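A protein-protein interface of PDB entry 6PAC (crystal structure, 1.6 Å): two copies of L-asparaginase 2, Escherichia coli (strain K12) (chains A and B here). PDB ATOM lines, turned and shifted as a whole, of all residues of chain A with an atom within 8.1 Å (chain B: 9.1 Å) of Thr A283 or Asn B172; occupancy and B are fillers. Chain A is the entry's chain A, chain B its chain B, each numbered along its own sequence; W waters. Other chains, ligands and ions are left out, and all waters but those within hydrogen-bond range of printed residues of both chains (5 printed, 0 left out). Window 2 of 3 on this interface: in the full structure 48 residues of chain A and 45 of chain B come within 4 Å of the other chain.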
ATOM      1  N   ASP A 167     -14.152  13.759  -0.068  1.00  0.00           N
ATOM      2  CA  ASP A 167     -15.386  13.939   0.668  1.00  0.00           C
ATOM      3  C   ASP A 167     -16.113  12.657   0.993  1.00  0.00           C
ATOM      4  O   ASP A 167     -16.955  12.611   1.861  1.00  0.00           O
ATOM      5  CB  ASP A 167     -16.316  14.939  -0.027  1.00  0.00           C
ATOM      6  CG  ASP A 167     -17.334  15.603   0.960  1.00  0.00           C
ATOM      7  OD1 ASP A 167     -16.899  16.010   2.074  1.00  0.00           O
ATOM      8  OD2 ASP A 167     -18.512  15.682   0.525  1.00  0.00           O
ATOM      9  N   THR A 169     -17.628   9.335   2.380  1.00  0.00           N
ATOM     10  CA  THR A 169     -17.613   8.697   3.728  1.00  0.00           C
ATOM     11  C   THR A 169     -18.699   7.675   3.829  1.00  0.00           C
ATOM     12  O   THR A 169     -19.709   7.698   3.089  1.00  0.00           O
ATOM     13  CB  THR A 169     -17.683   9.759   4.832  1.00  0.00           C
ATOM     14  OG1 THR A 169     -17.495   9.163   6.116  1.00  0.00           O
ATOM     15  CG2 THR A 169     -18.969  10.448   4.766  1.00  0.00           C
ATOM     16  N   THR A 171     -21.751   6.341   5.570  1.00  0.00           N
ATOM     17  CA  THR A 171     -22.741   6.977   6.389  1.00  0.00           C
ATOM     18  C   THR A 171     -23.613   6.048   7.215  1.00  0.00           C
ATOM     19  O   THR A 171     -24.224   6.515   8.195  1.00  0.00           O
ATOM     20  CB  THR A 171     -23.660   7.913   5.599  1.00  0.00           C
ATOM     21  OG1 THR A 171     -24.496   7.162   4.704  1.00  0.00           O
ATOM     22  CG2 THR A 171     -22.909   8.959   4.810  1.00  0.00           C
ATOM     23  N   SER A 181     -20.836  11.556  -0.387  1.00  0.00           N
ATOM     24  CA  SER A 181     -19.936  12.722  -0.210  1.00  0.00           C
ATOM     25  C   SER A 181     -20.822  13.781   0.472  1.00  0.00           C
ATOM     26  O   SER A 181     -21.599  14.563  -0.141  1.00  0.00           O
ATOM     27  CB  SER A 181     -19.405  13.158  -1.528  1.00  0.00           C
ATOM     28  OG  SER A 181     -18.399  12.269  -1.989  1.00  0.00           O
ATOM     29  N   VAL A 182     -20.779  13.723   1.781  1.00  0.00           N
ATOM     30  CA  VAL A 182     -21.801  14.367   2.561  1.00  0.00           C
ATOM     31  C   VAL A 182     -21.779  15.907   2.580  1.00  0.00           C
ATOM     32  O   VAL A 182     -22.818  16.509   2.924  1.00  0.00           O
ATOM     33  CB  VAL A 182     -21.768  13.844   4.001  1.00  0.00           C
ATOM     34  CG1 VAL A 182     -22.098  12.382   4.037  1.00  0.00           C
ATOM     35  CG2 VAL A 182     -20.445  14.060   4.698  1.00  0.00           C
ATOM     36  N   ASN A 183     -20.656  16.511   2.290  1.00  0.00           N
ATOM     37  CA  ASN A 183     -20.546  17.985   2.304  1.00  0.00           C
ATOM     38  C   ASN A 183     -20.698  18.594   0.922  1.00  0.00           C
ATOM     39  O   ASN A 183     -21.351  19.617   0.809  1.00  0.00           O
ATOM     40  CB  ASN A 183     -19.190  18.372   2.863  1.00  0.00           C
ATOM     41  CG  ASN A 183     -19.023  17.883   4.308  1.00  0.00           C
ATOM     42  OD1 ASN A 183     -19.802  18.304   5.171  1.00  0.00           O
ATOM     43  ND2 ASN A 183     -18.141  16.911   4.546  1.00  0.00           N
ATOM     44  N   GLY A 253     -19.299  19.045  18.677  1.00  0.00           N
ATOM     45  CA  GLY A 253     -19.690  20.184  17.894  1.00  0.00           C
ATOM     46  C   GLY A 253     -18.619  20.670  16.906  1.00  0.00           C
ATOM     47  O   GLY A 253     -18.013  19.902  16.128  1.00  0.00           O
ATOM     48  N   ASN A 254     -18.446  21.971  16.892  1.00  0.00           N
ATOM     49  CA  ASN A 254     -17.438  22.609  16.033  1.00  0.00           C
ATOM     50  C   ASN A 254     -16.025  22.442  16.571  1.00  0.00           C
ATOM     51  O   ASN A 254     -15.329  23.420  16.880  1.00  0.00           O
ATOM     52  CB  ASN A 254     -17.784  24.088  15.794  1.00  0.00           C
ATOM     53  CG  ASN A 254     -16.972  24.740  14.689  1.00  0.00           C
ATOM     54  OD1 ASN A 254     -16.008  24.151  14.077  1.00  0.00           O
ATOM     55  ND2 ASN A 254     -17.336  26.000  14.375  1.00  0.00           N
ATOM     56  N   SER A 279     -13.914  16.801  14.224  1.00  0.00           N
ATOM     57  CA  SER A 279     -15.221  16.737  14.903  1.00  0.00           C
ATOM     58  C   SER A 279     -15.774  15.315  14.738  1.00  0.00           C
ATOM     59  O   SER A 279     -15.764  14.761  13.595  1.00  0.00           O
ATOM     60  CB  SER A 279     -16.269  17.768  14.349  1.00  0.00           C
ATOM     61  OG  SER A 279     -17.433  17.532  15.078  1.00  0.00           O
ATOM     62  N   ARG A 280     -16.365  14.790  15.821  1.00  0.00           N
ATOM     63  CA  ARG A 280     -17.155  13.612  15.769  1.00  0.00           C
ATOM     64  C   ARG A 280     -18.461  13.787  15.019  1.00  0.00           C
ATOM     65  O   ARG A 280     -19.112  12.812  14.646  1.00  0.00           O
ATOM     66  CB  ARG A 280     -17.481  13.094  17.151  1.00  0.00           C
ATOM     67  CG  ARG A 280     -18.588  13.914  17.843  1.00  0.00           C
ATOM     68  CD  ARG A 280     -18.779  13.454  19.264  1.00  0.00           C
ATOM     69  NE  ARG A 280     -19.990  14.048  19.843  1.00  0.00           N
ATOM     70  CZ  ARG A 280     -20.418  13.825  21.089  1.00  0.00           C
ATOM     71  NH1 ARG A 280     -21.605  14.337  21.487  1.00  0.00           N
ATOM     72  NH2 ARG A 280     -19.647  13.166  21.960  1.00  0.00           N
ATOM     73  N   VAL A 281     -18.844  15.021  14.748  1.00  0.00           N
ATOM     74  CA  VAL A 281     -20.097  15.353  14.048  1.00  0.00           C
ATOM     75  C   VAL A 281     -19.900  15.004  12.557  1.00  0.00           C
ATOM     76  O   VAL A 281     -18.868  15.362  11.973  1.00  0.00           O
ATOM     77  CB  VAL A 281     -20.463  16.838  14.271  1.00  0.00           C
ATOM     78  CG1 VAL A 281     -21.639  17.261  13.440  1.00  0.00           C
ATOM     79  CG2 VAL A 281     -20.685  17.081  15.789  1.00  0.00           C
ATOM     80  N   PRO A 282     -20.870  14.338  11.948  1.00  0.00           N
ATOM     81  CA  PRO A 282     -20.603  13.641  10.656  1.00  0.00           C
ATOM     82  C   PRO A 282     -20.577  14.545   9.455  1.00  0.00           C
ATOM     83  O   PRO A 282     -20.102  14.093   8.398  1.00  0.00           O
ATOM     84  CB  PRO A 282     -21.733  12.610  10.540  1.00  0.00           C
ATOM     85  CG  PRO A 282     -22.838  13.170  11.391  1.00  0.00           C
ATOM     86  CD  PRO A 282     -22.116  13.848  12.561  1.00  0.00           C
ATOM     87  N   THR A 283     -21.082  15.769   9.557  1.00  0.00           N
ATOM     88  CA  THR A 283     -21.019  16.668   8.442  1.00  0.00           C
ATOM     89  C   THR A 283     -20.665  18.047   8.923  1.00  0.00           C
ATOM     90  O   THR A 283     -20.841  18.351  10.106  1.00  0.00           O
ATOM     91  CB  THR A 283     -22.339  16.754   7.627  1.00  0.00           C
ATOM     92  OG1 THR A 283     -23.332  17.528   8.333  1.00  0.00           O
ATOM     93  CG2 THR A 283     -22.892  15.412   7.289  1.00  0.00           C
ATOM     94  N   GLY A 284     -20.125  18.833   8.011  1.00  0.00           N
ATOM     95  CA  GLY A 284     -19.688  20.195   8.323  1.00  0.00           C
ATOM     96  C   GLY A 284     -18.253  20.381   8.727  1.00  0.00           C
ATOM     97  O   GLY A 284     -17.583  19.484   9.174  1.00  0.00           O
ATOM     98  N   ALA A 285     -17.786  21.603   8.548  1.00  0.00           N
ATOM     99  CA  ALA A 285     -16.406  21.908   8.885  1.00  0.00           C
ATOM    100  C   ALA A 285     -16.171  22.138  10.338  1.00  0.00           C
ATOM    101  O   ALA A 285     -17.004  22.703  11.052  1.00  0.00           O
ATOM    102  CB  ALA A 285     -15.905  23.132   8.100  1.00  0.00           C
ATOM    103  N   THR A 286     -14.967  21.747  10.782  1.00  0.00           N
ATOM    104  CA  THR A 286     -14.345  22.270  12.010  1.00  0.00           C
ATOM    105  C   THR A 286     -13.605  23.560  11.591  1.00  0.00           C
ATOM    106  O   THR A 286     -12.622  23.498  10.856  1.00  0.00           O
ATOM    107  CB  THR A 286     -13.437  21.294  12.677  1.00  0.00           C
ATOM    108  OG1 THR A 286     -14.197  20.177  13.090  1.00  0.00           O
ATOM    109  CG2 THR A 286     -12.711  21.951  13.845  1.00  0.00           C
ATOM    110  N   GLY A 303     -11.199  21.696   8.995  1.00  0.00           N
ATOM    111  CA  GLY A 303     -12.208  21.938   7.930  1.00  0.00           C
ATOM    112  C   GLY A 303     -13.149  20.713   7.830  1.00  0.00           C
ATOM    113  O   GLY A 303     -13.536  20.152   8.833  1.00  0.00           O
ATOM    114  N   THR A 304     -13.581  20.379   6.611  1.00  0.00           N
ATOM    115  CA  THR A 304     -14.565  19.338   6.458  1.00  0.00           C
ATOM    116  C   THR A 304     -13.971  17.946   6.634  1.00  0.00           C
ATOM    117  O   THR A 304     -14.722  16.958   6.587  1.00  0.00           O
ATOM    118  CB  THR A 304     -15.265  19.409   5.084  1.00  0.00           C
ATOM    119  OG1 THR A 304     -14.351  19.181   4.042  1.00  0.00           O
ATOM    120  CG2 THR A 304     -15.996  20.755   4.878  1.00  0.00           C
ATOM    121  N   ASN A 306     -13.123  14.831   8.369  1.00  0.00           N
ATOM    122  CA  ASN A 306     -13.472  14.068   9.533  1.00  0.00           C
ATOM    123  C   ASN A 306     -12.222  13.474  10.187  1.00  0.00           C
ATOM    124  O   ASN A 306     -11.110  13.627   9.658  1.00  0.00           O
ATOM    125  CB  ASN A 306     -14.588  13.086   9.207  1.00  0.00           C
ATOM    126  CG  ASN A 306     -14.158  11.900   8.386  1.00  0.00           C
ATOM    127  OD1 ASN A 306     -13.005  11.473   8.481  1.00  0.00           O
ATOM    128  ND2 ASN A 306     -15.102  11.294   7.659  1.00  0.00           N
ATOM    129  N   THR B  97     -25.325  22.815  22.663  1.00  0.00           N
ATOM    130  CA  THR B  97     -25.666  21.878  21.681  1.00  0.00           C
ATOM    131  C   THR B  97     -24.618  20.742  21.566  1.00  0.00           C
ATOM    132  O   THR B  97     -24.963  19.689  21.150  1.00  0.00           O
ATOM    133  CB  THR B  97     -25.820  22.531  20.316  1.00  0.00           C
ATOM    134  OG1 THR B  97     -24.559  23.072  19.888  1.00  0.00           O
ATOM    135  CG2 THR B  97     -26.875  23.647  20.331  1.00  0.00           C
ATOM    136  N   ASP B  98     -23.370  20.992  21.970  1.00  0.00           N
ATOM    137  CA  ASP B  98     -22.292  19.990  21.728  1.00  0.00           C
ATOM    138  C   ASP B  98     -22.538  18.624  22.346  1.00  0.00           C
ATOM    139  O   ASP B  98     -22.327  17.618  21.637  1.00  0.00           O
ATOM    140  CB  ASP B  98     -20.954  20.517  22.164  1.00  0.00           C
ATOM    141  CG  ASP B  98     -20.463  21.642  21.312  1.00  0.00           C
ATOM    142  OD1 ASP B  98     -21.096  21.972  20.291  1.00  0.00           O
ATOM    143  OD2 ASP B  98     -19.387  22.160  21.633  1.00  0.00           O
ATOM    144  N   GLU B 101     -27.165  15.805  23.085  1.00  0.00           N
ATOM    145  CA  GLU B 101     -27.666  14.481  22.803  1.00  0.00           C
ATOM    146  C   GLU B 101     -27.310  13.454  23.890  1.00  0.00           C
ATOM    147  O   GLU B 101     -27.933  12.410  23.933  1.00  0.00           O
ATOM    148  CB  GLU B 101     -27.150  13.993  21.460  1.00  0.00           C
ATOM    149  CG  GLU B 101     -25.660  13.556  21.455  1.00  0.00           C
ATOM    150  CD  GLU B 101     -25.075  13.509  20.011  1.00  0.00           C
ATOM    151  OE1 GLU B 101     -24.878  12.362  19.510  1.00  0.00           O
ATOM    152  OE2 GLU B 101     -24.897  14.579  19.392  1.00  0.00           O
ATOM    153  N   MET B 123     -27.740  27.232  18.038  1.00  0.00           N
ATOM    154  CA  MET B 123     -26.549  27.208  17.259  1.00  0.00           C
ATOM    155  C   MET B 123     -25.896  28.538  16.994  1.00  0.00           C
ATOM    156  O   MET B 123     -24.749  28.586  16.654  1.00  0.00           O
ATOM    157  CB  MET B 123     -26.841  26.435  15.928  1.00  0.00           C
ATOM    158  CG  MET B 123     -27.172  24.979  16.116  1.00  0.00           C
ATOM    159  SD  MET B 123     -25.750  24.033  16.739  1.00  0.00           S
ATOM    160  CE  MET B 123     -24.791  23.904  15.248  1.00  0.00           C
ATOM    161  N   THR B 169     -29.366  13.336  17.470  1.00  0.00           N
ATOM    162  CA  THR B 169     -27.936  13.580  17.408  1.00  0.00           C
ATOM    163  C   THR B 169     -27.629  14.838  16.620  1.00  0.00           C
ATOM    164  O   THR B 169     -28.426  15.279  15.799  1.00  0.00           O
ATOM    165  CB  THR B 169     -27.177  12.335  16.849  1.00  0.00           C
ATOM    166  OG1 THR B 169     -25.733  12.509  16.955  1.00  0.00           O
ATOM    167  CG2 THR B 169     -27.594  12.031  15.394  1.00  0.00           C
ATOM    168  N   LYS B 170     -26.499  15.432  16.913  1.00  0.00           N
ATOM    169  CA  LYS B 170     -25.995  16.599  16.176  1.00  0.00           C
ATOM    170  C   LYS B 170     -25.314  16.143  14.873  1.00  0.00           C
ATOM    171  O   LYS B 170     -24.266  15.492  14.947  1.00  0.00           O
ATOM    172  CB  LYS B 170     -25.060  17.419  17.086  1.00  0.00           C
ATOM    173  CG  LYS B 170     -24.625  18.740  16.510  1.00  0.00           C
ATOM    174  CD  LYS B 170     -23.931  19.610  17.579  1.00  0.00           C
ATOM    175  CE  LYS B 170     -23.409  20.860  17.046  1.00  0.00           C
ATOM    176  NZ  LYS B 170     -22.971  21.745  18.179  1.00  0.00           N
ATOM    177  N   THR B 171     -25.906  16.477  13.711  1.00  0.00           N
ATOM    178  CA  THR B 171     -25.441  15.970  12.418  1.00  0.00           C
ATOM    179  C   THR B 171     -24.503  16.905  11.665  1.00  0.00           C
ATOM    180  O   THR B 171     -23.754  16.423  10.758  1.00  0.00           O
ATOM    181  CB  THR B 171     -26.604  15.610  11.491  1.00  0.00           C
ATOM    182  OG1 THR B 171     -27.345  16.769  11.079  1.00  0.00           O
ATOM    183  CG2 THR B 171     -27.487  14.639  12.123  1.00  0.00           C
ATOM    184  N   ASN B 172     -24.520  18.197  12.011  1.00  0.00           N
ATOM    185  CA  ASN B 172     -23.731  19.202  11.367  1.00  0.00           C
ATOM    186  C   ASN B 172     -23.041  20.130  12.358  1.00  0.00           C
ATOM    187  O   ASN B 172     -23.586  20.525  13.358  1.00  0.00           O
ATOM    188  CB  ASN B 172     -24.569  19.990  10.347  1.00  0.00           C
ATOM    189  CG  ASN B 172     -23.737  20.924   9.489  1.00  0.00           C
ATOM    190  OD1 ASN B 172     -23.566  22.105   9.867  1.00  0.00           O
ATOM    191  ND2 ASN B 172     -23.124  20.411   8.405  1.00  0.00           N
ATOM    192  N   THR B 173     -21.841  20.564  12.046  1.00  0.00           N
ATOM    193  CA  THR B 173     -21.067  21.357  13.018  1.00  0.00           C
ATOM    194  C   THR B 173     -21.638  22.791  13.221  1.00  0.00           C
ATOM    195  O   THR B 173     -21.373  23.353  14.293  1.00  0.00           O
ATOM    196  CB  THR B 173     -19.603  21.525  12.579  1.00  0.00           C
ATOM    197  OG1 THR B 173     -19.553  22.033  11.237  1.00  0.00           O
ATOM    198  CG2 THR B 173     -18.891  20.223  12.695  1.00  0.00           C
ATOM    199  N   THR B 174     -22.377  23.378  12.250  1.00  0.00           N
ATOM    200  CA  THR B 174     -22.825  24.761  12.385  1.00  0.00           C
ATOM    201  C   THR B 174     -24.294  25.044  12.027  1.00  0.00           C
ATOM    202  O   THR B 174     -24.841  26.083  12.414  1.00  0.00           O
ATOM    203  CB  THR B 174     -21.937  25.660  11.532  1.00  0.00           C
ATOM    204  OG1 THR B 174     -22.115  25.342  10.144  1.00  0.00           O
ATOM    205  CG2 THR B 174     -20.457  25.562  11.958  1.00  0.00           C
ATOM    206  N   ASP B 175     -24.959  24.117  11.322  1.00  0.00           N
ATOM    207  CA  ASP B 175     -26.316  24.343  10.762  1.00  0.00           C
ATOM    208  C   ASP B 175     -27.338  24.470  11.888  1.00  0.00           C
ATOM    209  O   ASP B 175     -27.399  23.655  12.829  1.00  0.00           O
ATOM    210  CB  ASP B 175     -26.656  23.129   9.889  1.00  0.00           C
ATOM    211  CG  ASP B 175     -27.865  23.273   9.012  1.00  0.00           C
ATOM    212  OD1 ASP B 175     -28.803  24.032   9.254  1.00  0.00           O
ATOM    213  OD2 ASP B 175     -27.896  22.484   8.028  1.00  0.00           O
ATOM    214  N   VAL B 176     -28.188  25.468  11.803  1.00  0.00           N
ATOM    215  CA  VAL B 176     -29.303  25.529  12.726  1.00  0.00           C
ATOM    216  C   VAL B 176     -30.209  24.294  12.738  1.00  0.00           C
ATOM    217  O   VAL B 176     -30.873  24.052  13.765  1.00  0.00           O
ATOM    218  CB  VAL B 176     -30.184  26.813  12.568  1.00  0.00           C
ATOM    219  CG1 VAL B 176     -29.338  28.065  12.883  1.00  0.00           C
ATOM    220  CG2 VAL B 176     -30.790  26.904  11.167  1.00  0.00           C
ATOM    221  N   ALA B 177     -30.254  23.541  11.629  1.00  0.00           N
ATOM    222  CA  ALA B 177     -31.068  22.340  11.411  1.00  0.00           C
ATOM    223  C   ALA B 177     -30.325  21.069  11.796  1.00  0.00           C
ATOM    224  O   ALA B 177     -30.724  19.990  11.457  1.00  0.00           O
ATOM    225  CB  ALA B 177     -31.513  22.247   9.957  1.00  0.00           C
ATOM    226  N   THR B 178     -29.243  21.236  12.532  1.00  0.00           N
ATOM    227  CA  THR B 178     -28.337  20.152  12.831  1.00  0.00           C
ATOM    228  C   THR B 178     -28.929  18.929  13.526  1.00  0.00           C
ATOM    229  O   THR B 178     -28.521  17.773  13.236  1.00  0.00           O
ATOM    230  CB  THR B 178     -27.130  20.643  13.633  1.00  0.00           C
ATOM    231  OG1 THR B 178     -26.149  19.582  13.750  1.00  0.00           O
ATOM    232  CG2 THR B 178     -27.489  21.198  14.981  1.00  0.00           C
ATOM    233  N   PHE B 179     -29.830  19.149  14.485  1.00  0.00           N
ATOM    234  CA  PHE B 179     -30.349  18.037  15.252  1.00  0.00           C
ATOM    235  C   PHE B 179     -31.389  17.188  14.551  1.00  0.00           C
ATOM    236  O   PHE B 179     -32.417  17.750  14.075  1.00  0.00           O
ATOM    237  CB  PHE B 179     -30.925  18.508  16.589  1.00  0.00           C
ATOM    238  CG  PHE B 179     -29.869  18.842  17.572  1.00  0.00           C
ATOM    239  CD1 PHE B 179     -29.226  17.835  18.283  1.00  0.00           C
ATOM    240  CD2 PHE B 179     -29.479  20.122  17.743  1.00  0.00           C
ATOM    241  CE1 PHE B 179     -28.202  18.148  19.150  1.00  0.00           C
ATOM    242  CE2 PHE B 179     -28.457  20.458  18.634  1.00  0.00           C
ATOM    243  CZ  PHE B 179     -27.787  19.454  19.332  1.00  0.00           C
ATOM    244  N   LYS B 180     -31.121  15.892  14.413  1.00  0.00           N
ATOM    245  CA  LYS B 180     -31.997  14.975  13.698  1.00  0.00           C
ATOM    246  C   LYS B 180     -32.002  13.621  14.413  1.00  0.00           C
ATOM    247  O   LYS B 180     -30.983  13.268  15.055  1.00  0.00           O
ATOM    248  CB  LYS B 180     -31.455  14.719  12.307  1.00  0.00           C
ATOM    249  CG  LYS B 180     -31.461  15.921  11.382  1.00  0.00           C
ATOM    250  CD  LYS B 180     -32.946  16.291  11.056  1.00  0.00           C
ATOM    251  CE  LYS B 180     -33.193  17.098   9.792  1.00  0.00           C
ATOM    252  NZ  LYS B 180     -32.509  18.431   9.962  1.00  0.00           N
ATOM    253  N   VAL B 182     -31.716  10.380  13.370  1.00  0.00           N
ATOM    254  CA  VAL B 182     -31.197   9.918  12.100  1.00  0.00           C
ATOM    255  C   VAL B 182     -31.564   8.487  11.723  1.00  0.00           C
ATOM    256  O   VAL B 182     -31.498   8.138  10.559  1.00  0.00           O
ATOM    257  CB  VAL B 182     -29.647  10.054  12.039  1.00  0.00           C
ATOM    258  CG1 VAL B 182     -29.223  11.507  12.193  1.00  0.00           C
ATOM    259  CG2 VAL B 182     -28.979   9.182  13.115  1.00  0.00           C
ATOM    260  N   PRO B 282     -22.231   7.299  11.266  1.00  0.00           N
ATOM    261  CA  PRO B 282     -23.215   8.130  11.959  1.00  0.00           C
ATOM    262  C   PRO B 282     -24.603   7.593  11.971  1.00  0.00           C
ATOM    263  O   PRO B 282     -25.433   8.130  12.730  1.00  0.00           O
ATOM    264  CB  PRO B 282     -23.224   9.439  11.166  1.00  0.00           C
ATOM    265  CG  PRO B 282     -22.635   9.122   9.830  1.00  0.00           C
ATOM    266  CD  PRO B 282     -21.611   8.017  10.142  1.00  0.00           C
ATOM    267  N   THR B 283     -24.932   6.623  11.137  1.00  0.00           N
ATOM    268  CA  THR B 283     -26.252   6.053  11.152  1.00  0.00           C
ATOM    269  C   THR B 283     -26.170   4.530  11.050  1.00  0.00           C
ATOM    270  O   THR B 283     -25.212   3.992  10.513  1.00  0.00           O
ATOM    271  CB  THR B 283     -27.147   6.576  10.021  1.00  0.00           C
ATOM    272  OG1 THR B 283     -26.766   6.081   8.717  1.00  0.00           O
ATOM    273  CG2 THR B 283     -27.175   8.141  10.020  1.00  0.00           C
HETATM  274  O   HOH W   1     -21.438  17.283  19.162  1.00  0.00           O
HETATM  275  O   HOH W   2     -22.045  20.072   5.460  1.00  0.00           O
HETATM  276  O   HOH W   3     -19.846  23.758  18.621  1.00  0.00           O
HETATM  277  O   HOH W   4     -22.456  14.877  18.367  1.00  0.00           O
HETATM  278  O   HOH W   5     -20.362  23.701   8.995  1.00  0.00           O
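Among the printed residues, merely in contact across the chains: Gly A284 with Thr B173 (3.3 Å), Gly A253 with Asp B98 (3.3 Å), Val A281 with Asn B172 (3.3 Å), Val A281 with Thr B171 (3.4 Å), Pro A282 with Thr B171 (3.4 Å), Thr A171 with Pro B282 (3.5 Å), Val A281 with Lys B170 (3.5 Å), Gly A253 with Thr B173 (3.6 Å), Pro A282 with Pro B282 (3.6 Å), Val A281 with Thr B173 (3.6 Å), Pro A282 with Lys B170 (3.6 Å), Gly A253 with Lys B170 (3.6 Å), Ser A279 with Thr B173 (3.9 Å), Asn A254 with Thr B173 (3.96 Å) and Asn A254 with Thr B174 (3.97 Å).
Of chain B, only Thr B171 (2.7 Å), Asn B172 (2.9 Å) and Thr B173 (3.1 Å) come within 4 Å of Thr A283.
Asn B172 touches just these residues of chain A: Val A281, Thr A283 and Gly A284.
Of chain B, only Asn B172 and Thr B173 come within 4 Å of Gly A284.
Of the printed residues of chain A, Glu B101 touches Arg A280.
Printed residues of chain B within 4 Å of Ser A279: Thr B173 (3.9 Å).
Of the printed residues of chain B, Val A281 touches Lys B170 (3.5 Å), Thr B171 (3.4 Å), Asn B172 (3.3 Å) and Thr B173 (3.6 Å).
Printed residues of chain B within 4 Å of Arg A280: Asp B98 (3.4 Å) and Glu B101 (3.9 Å).
Printed residues of chain A within 4 Å of Lys B170: Gly A253 (3.6 Å), Val A281 (3.5 Å) and Pro A282 (3.6 Å).
Asn A183 touches none of the printed residues of chain B.
The nearest residue of chain B that does not touch Thr A283 is Thr B174 (5.7 Å).
The nearest residue of chain A that does not touch Asn B172 is Pro A282 (5.0 Å).
Water W1 bridges the backbone carbonyl oxygen of Asp B98 (2.7 Å) and the backbone NH of Gly A253 (2.8 Å).
Water W5 lies within hydrogen-bond range of the side-chain hydroxyl (OG1) of Thr B174 (2.7 Å), the side-chain hydroxyl (OG1) of Thr B173 (2.9 Å) and the backbone NH (N) of Ala A285 (3.4 Å).
Water W4 bridges the side-chain carboxylate of Glu B101 (2.7 Å) and the guanidinium group of Arg A280 (3.0 Å).
Water W3 lies within hydrogen-bond range of OD1 of Asp B98 (2.7 Å) and N of Asn A254 (2.9 Å).
Water W2 lies within hydrogen-bond range of OD1 of Asn A183 (2.9 Å), ND2 of Asn B172 (3.2 Å) and N of Gly A284 (3.4 Å).
Of the 19 printed residues of chain B, 9 touch a printed residue of chain A.
Printed residues of chain B that touch a printed residue of chain A: Asp B98, Glu B101, Lys B170, Thr B171, Asn B172, Thr B173, Thr B174, Pro B282 and Thr B283.
Hydrophobic or aromatic side chains of chain B within 4 Å of the printed part of chain A: Pro B282.
Printed residues of chain A that touch a printed residue of chain B: Thr A171, Gly A253, Asn A254, Ser A279, Arg A280, Val A281, Pro A282, Thr A283, Gly A284 and Ala A285.
Among the printed residues, Asp or Glu carboxylates within 4 Å of a Lys or Arg side-chain nitrogen of the other chain: Arg A280 with Glu B101.
Thr A171 touches Pro B282, and with the chains exchanged Pro A282 touches Thr B171.
Thr A171 touches Thr B283, and with the chains exchanged Thr A283 touches Thr B171.
Pro A282 touches its own counterpart, Pro B282.
Of the 23 pairs that touch across the chains among the printed residues, 5 have their exchanged pair printed and touching as well.
The side-chain amide nitrogen (ND2) of Asn B172 lies close to the backbone NH (N) of Gly A284, at 3.4 Å.
NH1 of Arg A280 is in hydrogen-bond range of O of Asp B98, 3.4 Å away.
O of Ala A285 is in hydrogen-bond range of OG1 of Thr B173, 2.6 Å away.
O of Thr A171 lies within hydrogen-bond range of OG1 of Thr B283 (2.6 Å).
The guanidinium group (NH1) of Arg A280 is in salt-bridge range of the side-chain carboxylate (OE2) of Glu B101.
The side-chain hydroxyl (OG1) of Thr A283 is in hydrogen-bond range of the side-chain amide nitrogen (ND2) of Asn B172 (2.9 Å).
O of Thr B171 lies within hydrogen-bond range of OG1 of Thr A283, at 2.7 Å.
The backbone carbonyl oxygen of Thr A283 sits at hydrogen-bond distance from the backbone NH of Thr B173 (3.1 Å).
OG1 of Thr B171 lies within hydrogen-bond range of O of Thr B178 (2.7 Å).
The side-chain amide oxygen (OD1) of Asn A254 lies close to the backbone carbonyl oxygen (O) of Ala A285 (3.5 Å).
The side-chain amide oxygen of Asn A183 sits at hydrogen-bond distance from the backbone NH of Gly A284 (2.9 Å).
O of Gly A253 lies within hydrogen-bond range of OG of Ser A279, at 2.7 Å.
The backbone NH (N) of Val A281 is in hydrogen-bond range of the side-chain hydroxyl (OG) of Ser A279, at 2.9 Å.
NZ of Lys B170 lies within hydrogen-bond range of OG1 of Thr B97 (2.7 Å).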
